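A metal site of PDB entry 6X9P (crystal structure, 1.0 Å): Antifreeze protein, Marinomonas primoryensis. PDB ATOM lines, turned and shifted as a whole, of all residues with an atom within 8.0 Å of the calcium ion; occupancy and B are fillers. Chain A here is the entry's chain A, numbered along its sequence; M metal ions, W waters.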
ATOM      1  N   TYR A  19      34.368  16.022  -2.193  1.00  0.00           N
ATOM      2  CA  TYR A  19      33.093  16.728  -2.143  1.00  0.00           C
ATOM      3  C   TYR A  19      33.338  18.156  -1.673  1.00  0.00           C
ATOM      4  O   TYR A  19      34.093  18.384  -0.717  1.00  0.00           O
ATOM      5  CB  TYR A  19      32.128  16.036  -1.162  1.00  0.00           C
ATOM      6  CG  TYR A  19      30.918  16.878  -0.878  1.00  0.00           C
ATOM      7  CD1 TYR A  19      29.871  16.975  -1.794  1.00  0.00           C
ATOM      8  CD2 TYR A  19      30.841  17.628   0.273  1.00  0.00           C
ATOM      9  CE1 TYR A  19      28.796  17.804  -1.569  1.00  0.00           C
ATOM     10  CE2 TYR A  19      29.761  18.478   0.501  1.00  0.00           C
ATOM     11  CZ  TYR A  19      28.738  18.558  -0.412  1.00  0.00           C
ATOM     12  OH  TYR A  19      27.653  19.384  -0.223  1.00  0.00           O
ATOM     13  N   VAL A  59      21.482  18.085  -2.490  1.00  0.00           N
ATOM     14  CA  VAL A  59      22.502  17.098  -2.133  1.00  0.00           C
ATOM     15  C   VAL A  59      23.296  17.561  -0.924  1.00  0.00           C
ATOM     16  O   VAL A  59      23.824  16.734  -0.176  1.00  0.00           O
ATOM     17  CB  VAL A  59      23.452  16.772  -3.315  1.00  0.00           C
ATOM     18  CG1 VAL A  59      24.573  17.789  -3.471  1.00  0.00           C
ATOM     19  CG2 VAL A  59      24.037  15.376  -3.143  1.00  0.00           C
ATOM     20  N   ALA A  60      23.425  18.871  -0.744  1.00  0.00           N
ATOM     21  CA  ALA A  60      24.344  19.445   0.236  1.00  0.00           C
ATOM     22  C   ALA A  60      23.729  19.580   1.618  1.00  0.00           C
ATOM     23  O   ALA A  60      24.425  20.025   2.547  1.00  0.00           O
ATOM     24  CB  ALA A  60      24.863  20.797  -0.293  1.00  0.00           C
ATOM     25  N   LYS A  61      22.476  19.200   1.803  1.00  0.00           N
ATOM     26  CA  LYS A  61      21.819  19.346   3.101  1.00  0.00           C
ATOM     27  C   LYS A  61      21.660  17.991   3.786  1.00  0.00           C
ATOM     28  O   LYS A  61      21.444  16.955   3.140  1.00  0.00           O
ATOM     29  CB  LYS A  61      20.501  20.137   2.971  1.00  0.00           C
ATOM     30  CG  LYS A  61      20.730  21.711   3.046  1.00  0.00           C
ATOM     31  CD  LYS A  61      20.130  22.524   1.885  1.00  0.00           C
ATOM     32  CE  LYS A  61      19.077  23.537   2.349  1.00  0.00           C
ATOM     33  NZ  LYS A  61      19.468  24.326   3.539  1.00  0.00           N
ATOM     34  N   GLY A  62      21.784  18.008   5.111  1.00  0.00           N
ATOM     35  CA  GLY A  62      21.539  16.826   5.937  1.00  0.00           C
ATOM     36  C   GLY A  62      22.405  15.662   5.538  1.00  0.00           C
ATOM     37  O   GLY A  62      23.623  15.805   5.353  1.00  0.00           O
ATOM     38  N   THR A  63      21.767  14.496   5.441  1.00  0.00           N
ATOM     39  CA  THR A  63      22.432  13.252   5.063  1.00  0.00           C
ATOM     40  C   THR A  63      22.234  12.916   3.594  1.00  0.00           C
ATOM     41  O   THR A  63      22.432  11.772   3.183  1.00  0.00           O
ATOM     42  CB  THR A  63      21.982  12.107   5.951  1.00  0.00           C
ATOM     43  OG1 THR A  63      20.565  11.913   5.821  1.00  0.00           O
ATOM     44  CG2 THR A  63      22.286  12.400   7.412  1.00  0.00           C
ATOM     45  N   HIS A  64      21.871  13.901   2.782  1.00  0.00           N
ATOM     46  CA  HIS A  64      21.595  13.607   1.373  1.00  0.00           C
ATOM     47  C   HIS A  64      22.833  13.156   0.618  1.00  0.00           C
ATOM     48  O   HIS A  64      22.729  12.319  -0.275  1.00  0.00           O
ATOM     49  CB  HIS A  64      20.932  14.806   0.717  1.00  0.00           C
ATOM     50  CG  HIS A  64      19.598  15.110   1.317  1.00  0.00           C
ATOM     51  ND1 HIS A  64      19.010  16.353   1.230  1.00  0.00           N
ATOM     52  CD2 HIS A  64      18.760  14.345   2.055  1.00  0.00           C
ATOM     53  CE1 HIS A  64      17.876  16.341   1.888  1.00  0.00           C
ATOM     54  NE2 HIS A  64      17.684  15.135   2.388  1.00  0.00           N
ATOM     55  N   LEU A  65      24.026  13.677   0.963  1.00  0.00           N
ATOM     56  CA  LEU A  65      25.229  13.245   0.278  1.00  0.00           C
ATOM     57  C   LEU A  65      25.483  11.769   0.524  1.00  0.00           C
ATOM     58  O   LEU A  65      25.871  11.029  -0.383  1.00  0.00           O
ATOM     59  CB  LEU A  65      26.424  14.072   0.723  1.00  0.00           C
ATOM     60  CG  LEU A  65      27.758  13.671   0.118  1.00  0.00           C
ATOM     61  CD1 LEU A  65      27.797  13.906  -1.376  1.00  0.00           C
ATOM     62  CD2 LEU A  65      28.890  14.414   0.817  1.00  0.00           C
ATOM     63  N   GLN A  66      25.317  11.356   1.773  1.00  0.00           N
ATOM     64  CA  GLN A  66      25.490   9.944   2.149  1.00  0.00           C
ATOM     65  C   GLN A  66      24.560   9.060   1.328  1.00  0.00           C
ATOM     66  O   GLN A  66      24.954   8.007   0.827  1.00  0.00           O
ATOM     67  CB  GLN A  66      25.188   9.760   3.638  1.00  0.00           C
ATOM     68  CG  GLN A  66      26.262  10.247   4.585  1.00  0.00           C
ATOM     69  CD  GLN A  66      26.291  11.746   4.865  1.00  0.00           C
ATOM     70  OE1 GLN A  66      25.534  12.553   4.307  1.00  0.00           O
ATOM     71  NE2 GLN A  66      27.210  12.132   5.722  1.00  0.00           N
ATOM     72  N   LEU A  76      33.571   8.046   3.442  1.00  0.00           N
ATOM     73  CA  LEU A  76      33.642   9.479   3.699  1.00  0.00           C
ATOM     74  C   LEU A  76      34.576   9.804   4.852  1.00  0.00           C
ATOM     75  O   LEU A  76      34.512   9.189   5.930  1.00  0.00           O
ATOM     76  CB  LEU A  76      32.255  10.057   4.020  1.00  0.00           C
ATOM     77  CG  LEU A  76      31.354  10.335   2.819  1.00  0.00           C
ATOM     78  CD1 LEU A  76      29.912  10.468   3.256  1.00  0.00           C
ATOM     79  CD2 LEU A  76      31.818  11.589   2.069  1.00  0.00           C
ATOM     80  N   THR A  78      34.519  12.593   6.555  1.00  0.00           N
ATOM     81  CA  THR A  78      33.758  13.377   7.510  1.00  0.00           C
ATOM     82  C   THR A  78      32.347  13.506   6.964  1.00  0.00           C
ATOM     83  O   THR A  78      32.097  13.236   5.787  1.00  0.00           O
ATOM     84  CB  THR A  78      34.445  14.731   7.746  1.00  0.00           C
ATOM     85  OG1 THR A  78      33.862  15.384   8.885  1.00  0.00           O
ATOM     86  CG2 THR A  78      34.312  15.614   6.527  1.00  0.00           C
ATOM     87  N   ASP A  79      31.422  13.935   7.831  1.00  0.00           N
ATOM     88  CA  ASP A  79      30.054  14.273   7.428  1.00  0.00           C
ATOM     89  C   ASP A  79      30.006  15.786   7.252  1.00  0.00           C
ATOM     90  O   ASP A  79      30.027  16.512   8.257  1.00  0.00           O
ATOM     91  CB  ASP A  79      29.080  13.828   8.522  1.00  0.00           C
ATOM     92  CG  ASP A  79      27.644  14.219   8.245  1.00  0.00           C
ATOM     93  OD1 ASP A  79      27.351  14.751   7.146  1.00  0.00           O
ATOM     94  OD2 ASP A  79      26.801  13.961   9.146  1.00  0.00           O
ATOM     95  N   PRO A  80      29.950  16.307   6.029  1.00  0.00           N
ATOM     96  CA  PRO A  80      29.895  17.763   5.844  1.00  0.00           C
ATOM     97  C   PRO A  80      28.676  18.363   6.532  1.00  0.00           C
ATOM     98  O   PRO A  80      27.622  17.742   6.644  1.00  0.00           O
ATOM     99  CB  PRO A  80      29.816  17.951   4.313  1.00  0.00           C
ATOM    100  CG  PRO A  80      30.214  16.656   3.717  1.00  0.00           C
ATOM    101  CD  PRO A  80      29.870  15.579   4.742  1.00  0.00           C
ATOM    102  N   GLY A  81      28.835  19.608   6.958  1.00  0.00           N
ATOM    103  CA  GLY A  81      27.689  20.408   7.385  1.00  0.00           C
ATOM    104  C   GLY A  81      26.823  20.809   6.195  1.00  0.00           C
ATOM    105  O   GLY A  81      27.077  20.481   5.040  1.00  0.00           O
ATOM    106  N   ASP A  82      25.730  21.514   6.503  1.00  0.00           N
ATOM    107  CA  ASP A  82      24.793  21.903   5.467  1.00  0.00           C
ATOM    108  C   ASP A  82      25.386  22.988   4.567  1.00  0.00           C
ATOM    109  O   ASP A  82      26.058  23.915   5.027  1.00  0.00           O
ATOM    110  CB  ASP A  82      23.516  22.481   6.075  1.00  0.00           C
ATOM    111  CG  ASP A  82      22.551  21.461   6.623  1.00  0.00           C
ATOM    112  OD1 ASP A  82      22.793  20.252   6.518  1.00  0.00           O
ATOM    113  OD2 ASP A  82      21.510  21.918   7.160  1.00  0.00           O
ATOM    114  N   ASN A  83      25.052  22.898   3.290  1.00  0.00           N
ATOM    115  CA  ASN A  83      25.245  23.972   2.313  1.00  0.00           C
ATOM    116  C   ASN A  83      24.031  23.963   1.393  1.00  0.00           C
ATOM    117  O   ASN A  83      23.268  22.986   1.374  1.00  0.00           O
ATOM    118  CB  ASN A  83      26.531  23.791   1.488  1.00  0.00           C
ATOM    119  CG  ASN A  83      27.787  24.217   2.208  1.00  0.00           C
ATOM    120  OD1 ASN A  83      27.977  25.433   2.467  1.00  0.00           O
ATOM    121  ND2 ASN A  83      28.654  23.311   2.480  1.00  0.00           N
HETATM  122 CA    CA M   1      25.733  16.434   6.316  1.00  0.00          CA
HETATM  123  O   HOH W   1      24.586  18.235   7.392  1.00  0.00           O
HETATM  124  O   HOH W   2      25.673  18.074   4.528  1.00  0.00           O
HETATM  125  O   HOH W   3      24.691  15.329   8.117  1.00  0.00           O
HETATM  126  O   HOH W   4      26.316  15.218   4.309  1.00  0.00           O
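The backbone NH of Gly 62 sits at hydrogen-bond distance from the side-chain carboxylate of Asp 82, 2.8 Å away.
The side-chain amide nitrogen (NE2) of Gln 66 lies close to the side-chain carboxylate (OD1) of Asp 79.
The nearest printed residue that does not touch the calcium ion is Gln 66 (4.4 Å).
Water W2 bridges O of Gly 81 (2.8 Å) and O of Ala 60 (3.0 Å).
The calcium ion is bound by O of Pro 80, water W3, water W1, O of Gly 62, water W4, water W2 and OD1 of Asp 79.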
